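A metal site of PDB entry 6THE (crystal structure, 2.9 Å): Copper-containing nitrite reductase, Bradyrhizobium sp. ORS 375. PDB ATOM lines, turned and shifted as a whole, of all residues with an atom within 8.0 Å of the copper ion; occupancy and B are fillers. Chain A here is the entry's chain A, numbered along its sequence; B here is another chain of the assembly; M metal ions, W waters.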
ATOM      1  N   ASP A  87       6.815   2.966   0.994  1.00  0.00           N
ATOM      2  CA  ASP A  87       6.368   3.722   2.153  1.00  0.00           C
ATOM      3  C   ASP A  87       5.936   2.741   3.242  1.00  0.00           C
ATOM      4  O   ASP A  87       4.970   2.001   3.057  1.00  0.00           O
ATOM      5  CB  ASP A  87       5.251   4.700   1.761  1.00  0.00           C
ATOM      6  CG  ASP A  87       4.531   5.363   2.924  1.00  0.00           C
ATOM      7  OD1 ASP A  87       5.000   5.242   4.080  1.00  0.00           O
ATOM      8  OD2 ASP A  87       3.501   6.014   2.665  1.00  0.00           O
ATOM      9  N   PHE A  88       6.671   2.748   4.363  1.00  0.00           N
ATOM     10  CA  PHE A  88       6.359   1.892   5.497  1.00  0.00           C
ATOM     11  C   PHE A  88       5.520   2.665   6.506  1.00  0.00           C
ATOM     12  O   PHE A  88       5.864   3.784   6.879  1.00  0.00           O
ATOM     13  CB  PHE A  88       7.643   1.361   6.135  1.00  0.00           C
ATOM     14  CG  PHE A  88       8.522   0.516   5.242  1.00  0.00           C
ATOM     15  CD1 PHE A  88       8.264  -0.838   5.081  1.00  0.00           C
ATOM     16  CD2 PHE A  88       9.591   1.070   4.567  1.00  0.00           C
ATOM     17  CE1 PHE A  88       9.060  -1.620   4.253  1.00  0.00           C
ATOM     18  CE2 PHE A  88      10.391   0.295   3.745  1.00  0.00           C
ATOM     19  CZ  PHE A  88      10.131  -1.045   3.588  1.00  0.00           C
ATOM     20  N   HIS A  89       4.409   2.046   6.925  1.00  0.00           N
ATOM     21  CA  HIS A  89       3.520   2.634   7.924  1.00  0.00           C
ATOM     22  C   HIS A  89       4.088   2.422   9.322  1.00  0.00           C
ATOM     23  O   HIS A  89       3.604   3.011  10.284  1.00  0.00           O
ATOM     24  CB  HIS A  89       2.104   2.045   7.787  1.00  0.00           C
ATOM     25  CG  HIS A  89       1.321   2.583   6.643  1.00  0.00           C
ATOM     26  ND1 HIS A  89      -0.037   2.811   6.729  1.00  0.00           N
ATOM     27  CD2 HIS A  89       1.681   2.952   5.391  1.00  0.00           C
ATOM     28  CE1 HIS A  89      -0.474   3.292   5.583  1.00  0.00           C
ATOM     29  NE2 HIS A  89       0.558   3.384   4.739  1.00  0.00           N
ATOM     30  N   GLY A  95       7.540  10.623   4.267  1.00  0.00           N
ATOM     31  CA  GLY A  95       7.032   9.754   3.220  1.00  0.00           C
ATOM     32  C   GLY A  95       7.101   8.286   3.611  1.00  0.00           C
ATOM     33  O   GLY A  95       6.949   7.411   2.758  1.00  0.00           O
ATOM     34  N   GLY A  96       7.344   8.014   4.899  1.00  0.00           N
ATOM     35  CA  GLY A  96       7.526   6.666   5.410  1.00  0.00           C
ATOM     36  C   GLY A  96       8.840   6.054   4.947  1.00  0.00           C
ATOM     37  O   GLY A  96       8.982   4.834   4.896  1.00  0.00           O
ATOM     38  N   VAL A 122       0.951  -1.578   6.841  1.00  0.00           N
ATOM     39  CA  VAL A 122       0.927  -1.689   5.390  1.00  0.00           C
ATOM     40  C   VAL A 122       2.175  -0.990   4.846  1.00  0.00           C
ATOM     41  O   VAL A 122       2.618   0.019   5.384  1.00  0.00           O
ATOM     42  CB  VAL A 122      -0.367  -1.091   4.799  1.00  0.00           C
ATOM     43  CG1 VAL A 122      -0.334  -1.002   3.273  1.00  0.00           C
ATOM     44  CG2 VAL A 122      -1.609  -1.836   5.260  1.00  0.00           C
ATOM     45  N   TYR A 123       2.744  -1.558   3.774  1.00  0.00           N
ATOM     46  CA  TYR A 123       3.736  -0.840   2.974  1.00  0.00           C
ATOM     47  C   TYR A 123       3.291  -0.826   1.517  1.00  0.00           C
ATOM     48  O   TYR A 123       2.583  -1.733   1.071  1.00  0.00           O
ATOM     49  CB  TYR A 123       5.155  -1.380   3.214  1.00  0.00           C
ATOM     50  CG  TYR A 123       5.499  -2.698   2.548  1.00  0.00           C
ATOM     51  CD1 TYR A 123       5.724  -2.775   1.188  1.00  0.00           C
ATOM     52  CD2 TYR A 123       5.632  -3.856   3.303  1.00  0.00           C
ATOM     53  CE1 TYR A 123       6.059  -3.976   0.578  1.00  0.00           C
ATOM     54  CE2 TYR A 123       5.965  -5.063   2.717  1.00  0.00           C
ATOM     55  CZ  TYR A 123       6.183  -5.123   1.344  1.00  0.00           C
ATOM     56  OH  TYR A 123       6.506  -6.310   0.757  1.00  0.00           O
ATOM     57  N   HIS A 124       3.712   0.213   0.788  1.00  0.00           N
ATOM     58  CA  HIS A 124       3.321   0.414  -0.600  1.00  0.00           C
ATOM     59  C   HIS A 124       4.290   1.385  -1.272  1.00  0.00           C
ATOM     60  O   HIS A 124       5.021   2.102  -0.607  1.00  0.00           O
ATOM     61  CB  HIS A 124       1.871   0.897  -0.696  1.00  0.00           C
ATOM     62  CG  HIS A 124       1.619   2.179   0.047  1.00  0.00           C
ATOM     63  ND1 HIS A 124       1.800   3.415  -0.530  1.00  0.00           N
ATOM     64  CD2 HIS A 124       1.197   2.402   1.312  1.00  0.00           C
ATOM     65  CE1 HIS A 124       1.514   4.353   0.346  1.00  0.00           C
ATOM     66  NE2 HIS A 124       1.135   3.755   1.488  1.00  0.00           N
ATOM     67  N   CYS A 125       4.268   1.396  -2.615  1.00  0.00           N
ATOM     68  CA  CYS A 125       5.030   2.347  -3.405  1.00  0.00           C
ATOM     69  C   CYS A 125       4.401   3.729  -3.263  1.00  0.00           C
ATOM     70  O   CYS A 125       3.174   3.867  -3.309  1.00  0.00           O
ATOM     71  CB  CYS A 125       5.049   1.930  -4.876  1.00  0.00           C
ATOM     72  SG  CYS A 125       6.082   2.981  -5.915  1.00  0.00           S
ATOM     73  N   ALA A 126       5.253   4.752  -3.115  1.00  0.00           N
ATOM     74  CA  ALA A 126       4.804   6.123  -2.934  1.00  0.00           C
ATOM     75  C   ALA A 126       5.425   7.019  -4.006  1.00  0.00           C
ATOM     76  O   ALA A 126       6.013   8.050  -3.680  1.00  0.00           O
ATOM     77  CB  ALA A 126       5.125   6.595  -1.534  1.00  0.00           C
ATOM     78  N   VAL A 130       0.505   7.851  -6.755  1.00  0.00           N
ATOM     79  CA  VAL A 130       0.647   6.812  -5.748  1.00  0.00           C
ATOM     80  C   VAL A 130      -0.476   5.787  -5.896  1.00  0.00           C
ATOM     81  O   VAL A 130      -0.245   4.590  -5.723  1.00  0.00           O
ATOM     82  CB  VAL A 130       0.703   7.412  -4.330  1.00  0.00           C
ATOM     83  CG1 VAL A 130       0.872   6.340  -3.258  1.00  0.00           C
ATOM     84  CG2 VAL A 130       1.789   8.464  -4.204  1.00  0.00           C
ATOM     85  N   ILE A 134       0.018   1.597  -6.335  1.00  0.00           N
ATOM     86  CA  ILE A 134      -0.608   0.682  -5.400  1.00  0.00           C
ATOM     87  C   ILE A 134      -1.538  -0.259  -6.162  1.00  0.00           C
ATOM     88  O   ILE A 134      -1.475  -1.474  -5.989  1.00  0.00           O
ATOM     89  CB  ILE A 134      -1.342   1.448  -4.275  1.00  0.00           C
ATOM     90  CG1 ILE A 134      -0.369   2.289  -3.434  1.00  0.00           C
ATOM     91  CG2 ILE A 134      -2.147   0.490  -3.402  1.00  0.00           C
ATOM     92  CD1 ILE A 134      -1.058   3.277  -2.511  1.00  0.00           C
ATOM     93  N   GLY A 221      -4.581  -3.161   0.542  1.00  0.00           N
ATOM     94  CA  GLY A 221      -3.776  -2.337  -0.332  1.00  0.00           C
ATOM     95  C   GLY A 221      -4.598  -1.195  -0.913  1.00  0.00           C
ATOM     96  O   GLY A 221      -4.136  -0.059  -0.971  1.00  0.00           O
ATOM     97  N   PRO A 260      -8.562   1.276   3.669  1.00  0.00           N
ATOM     98  CA  PRO A 260      -7.415   1.229   2.756  1.00  0.00           C
ATOM     99  C   PRO A 260      -6.174   1.753   3.476  1.00  0.00           C
ATOM    100  O   PRO A 260      -6.225   2.773   4.145  1.00  0.00           O
ATOM    101  CB  PRO A 260      -7.819   2.149   1.598  1.00  0.00           C
ATOM    102  CG  PRO A 260      -8.924   3.024   2.157  1.00  0.00           C
ATOM    103  CD  PRO A 260      -9.632   2.153   3.178  1.00  0.00           C
ATOM    104  N   GLY A 261      -5.070   1.004   3.343  1.00  0.00           N
ATOM    105  CA  GLY A 261      -3.836   1.308   4.048  1.00  0.00           C
ATOM    106  C   GLY A 261      -3.884   0.898   5.511  1.00  0.00           C
ATOM    107  O   GLY A 261      -2.995   1.233   6.292  1.00  0.00           O
ATOM    108  N   GLY A 262      -4.943   0.146   5.878  1.00  0.00           N
ATOM    109  CA  GLY A 262      -5.129  -0.346   7.229  1.00  0.00           C
ATOM    110  C   GLY A 262      -4.967  -1.863   7.294  1.00  0.00           C
ATOM    111  O   GLY A 262      -4.835  -2.520   6.264  1.00  0.00           O
ATOM    112  N   HIS B 230      -4.740   9.238   7.788  1.00  0.00           N
ATOM    113  CA  HIS B 230      -3.363   8.780   7.872  1.00  0.00           C
ATOM    114  C   HIS B 230      -2.424   9.958   7.606  1.00  0.00           C
ATOM    115  O   HIS B 230      -2.559  10.650   6.599  1.00  0.00           O
ATOM    116  CB  HIS B 230      -3.138   7.618   6.891  1.00  0.00           C
ATOM    117  CG  HIS B 230      -1.713   7.190   6.767  1.00  0.00           C
ATOM    118  ND1 HIS B 230      -1.120   6.322   7.652  1.00  0.00           N
ATOM    119  CD2 HIS B 230      -0.759   7.513   5.855  1.00  0.00           C
ATOM    120  CE1 HIS B 230       0.134   6.124   7.295  1.00  0.00           C
ATOM    121  NE2 HIS B 230       0.377   6.840   6.196  1.00  0.00           N
ATOM    122  N   VAL B 231      -1.484  10.171   8.533  1.00  0.00           N
ATOM    123  CA  VAL B 231      -0.382  11.079   8.323  1.00  0.00           C
ATOM    124  C   VAL B 231       0.806  10.276   7.810  1.00  0.00           C
ATOM    125  O   VAL B 231       1.304   9.396   8.511  1.00  0.00           O
ATOM    126  CB  VAL B 231      -0.029  11.867   9.604  1.00  0.00           C
ATOM    127  CG1 VAL B 231       1.178  12.769   9.414  1.00  0.00           C
ATOM    128  CG2 VAL B 231      -1.219  12.684  10.121  1.00  0.00           C
ATOM    129  N   ILE B 232       1.225  10.563   6.575  1.00  0.00           N
ATOM    130  CA  ILE B 232       2.279   9.814   5.914  1.00  0.00           C
ATOM    131  C   ILE B 232       3.613  10.124   6.611  1.00  0.00           C
ATOM    132  O   ILE B 232       4.060  11.263   6.624  1.00  0.00           O
ATOM    133  CB  ILE B 232       2.337  10.106   4.395  1.00  0.00           C
ATOM    134  CG1 ILE B 232       0.993   9.840   3.721  1.00  0.00           C
ATOM    135  CG2 ILE B 232       3.467   9.318   3.743  1.00  0.00           C
ATOM    136  CD1 ILE B 232       1.002  10.060   2.215  1.00  0.00           C
ATOM    137  N   GLY B 233       4.207   9.079   7.188  1.00  0.00           N
ATOM    138  CA  GLY B 233       5.485   9.177   7.860  1.00  0.00           C
ATOM    139  C   GLY B 233       5.346   9.158   9.380  1.00  0.00           C
ATOM    140  O   GLY B 233       6.344   9.278  10.096  1.00  0.00           O
ATOM    141  N   GLN B 254      -2.063   3.129  12.546  1.00  0.00           N
ATOM    142  CA  GLN B 254      -1.553   3.660  11.296  1.00  0.00           C
ATOM    143  C   GLN B 254      -2.638   4.480  10.604  1.00  0.00           C
ATOM    144  O   GLN B 254      -2.411   5.640  10.256  1.00  0.00           O
ATOM    145  CB  GLN B 254      -1.020   2.531  10.401  1.00  0.00           C
ATOM    146  CG  GLN B 254      -2.027   1.423  10.139  1.00  0.00           C
ATOM    147  CD  GLN B 254      -1.477   0.282   9.311  1.00  0.00           C
ATOM    148  OE1 GLN B 254      -0.716   0.476   8.372  1.00  0.00           O
ATOM    149  NE2 GLN B 254      -1.882  -0.936   9.660  1.00  0.00           N
ATOM    150  N   THR B 255      -3.814   3.869  10.415  1.00  0.00           N
ATOM    151  CA  THR B 255      -4.915   4.465   9.685  1.00  0.00           C
ATOM    152  C   THR B 255      -6.210   4.254  10.474  1.00  0.00           C
ATOM    153  O   THR B 255      -6.491   3.141  10.919  1.00  0.00           O
ATOM    154  CB  THR B 255      -5.005   3.890   8.262  1.00  0.00           C
ATOM    155  OG1 THR B 255      -3.720   3.966   7.657  1.00  0.00           O
ATOM    156  CG2 THR B 255      -6.009   4.606   7.389  1.00  0.00           C
ATOM    157  N   VAL B 279      -3.483  12.754   4.475  1.00  0.00           N
ATOM    158  CA  VAL B 279      -4.303  12.214   3.405  1.00  0.00           C
ATOM    159  C   VAL B 279      -5.368  11.284   3.984  1.00  0.00           C
ATOM    160  O   VAL B 279      -5.179  10.718   5.060  1.00  0.00           O
ATOM    161  CB  VAL B 279      -3.470  11.473   2.349  1.00  0.00           C
ATOM    162  CG1 VAL B 279      -2.706  12.407   1.416  1.00  0.00           C
ATOM    163  CG2 VAL B 279      -2.539  10.435   2.957  1.00  0.00           C
ATOM    164  N   HIS B 281      -6.656   7.677   3.011  1.00  0.00           N
ATOM    165  CA  HIS B 281      -5.873   6.620   2.390  1.00  0.00           C
ATOM    166  C   HIS B 281      -6.614   6.005   1.205  1.00  0.00           C
ATOM    167  O   HIS B 281      -6.144   5.044   0.603  1.00  0.00           O
ATOM    168  CB  HIS B 281      -5.370   5.615   3.431  1.00  0.00           C
ATOM    169  CG  HIS B 281      -3.995   5.111   3.148  1.00  0.00           C
ATOM    170  ND1 HIS B 281      -3.741   4.195   2.157  1.00  0.00           N
ATOM    171  CD2 HIS B 281      -2.803   5.403   3.716  1.00  0.00           C
ATOM    172  CE1 HIS B 281      -2.448   3.936   2.113  1.00  0.00           C
ATOM    173  NE2 HIS B 281      -1.847   4.667   3.073  1.00  0.00           N
ATOM    174  N   LEU B 283      -6.496   7.054  -1.885  1.00  0.00           N
ATOM    175  CA  LEU B 283      -5.478   7.995  -2.333  1.00  0.00           C
ATOM    176  C   LEU B 283      -5.745   8.495  -3.753  1.00  0.00           C
ATOM    177  O   LEU B 283      -4.925   9.223  -4.309  1.00  0.00           O
ATOM    178  CB  LEU B 283      -4.103   7.348  -2.205  1.00  0.00           C
ATOM    179  CG  LEU B 283      -3.519   7.305  -0.791  1.00  0.00           C
ATOM    180  CD1 LEU B 283      -2.386   6.301  -0.700  1.00  0.00           C
ATOM    181  CD2 LEU B 283      -3.045   8.686  -0.350  1.00  0.00           C
HETATM  182 CU    CU M   1       0.343   4.695   3.105  1.00  0.00          CU
HETATM  183  O   HOH W   1       0.865   6.624   2.943  1.00  0.00           O
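ND1 of His 89 lies close to O of Gly 261, 3.4 Å away.
The backbone carbonyl oxygen of His 230 of chain B sits at hydrogen-bond distance from the backbone NH of Val 279 of chain B, 3.1 Å away.
The backbone carbonyl oxygen of Pro 260 lies close to a ring nitrogen (ND1) of His 281 of chain B, at 3.5 Å.
The backbone NH of His 89 lies close to the backbone carbonyl oxygen of Val 122, at 3.1 Å.
The backbone carbonyl oxygen (O) of Gln 254 of chain B is in hydrogen-bond range of a ring nitrogen (ND1) of His 230 of chain B (3.0 Å).
The backbone carbonyl oxygen of His 124 sits at hydrogen-bond distance from the backbone NH of Asp 87, at 2.6 Å.
The side-chain amide oxygen (OE1) of Gln 254 of chain B is in hydrogen-bond range of a ring nitrogen (ND1) of His 89.
The copper ion is bound by water W1 (2.0 Å), NE2 of His 124 (2.0 Å), NE2 of His 89 (2.1 Å) and NE2 of His 281 of chain B (2.2 Å).
Asp 87 touches the copper ion (OD2 to CU, 3.5 Å).
His 230 of chain B touches the copper ion.
Five residues have an atom within 4 Å of the copper ion: Asp 87, His 89, His 124, His 230 of chain B and His 281 of chain B.
Water W1 lies within hydrogen-bond range of OD2 of Asp 87 and NE2 of His 230 of chain B.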
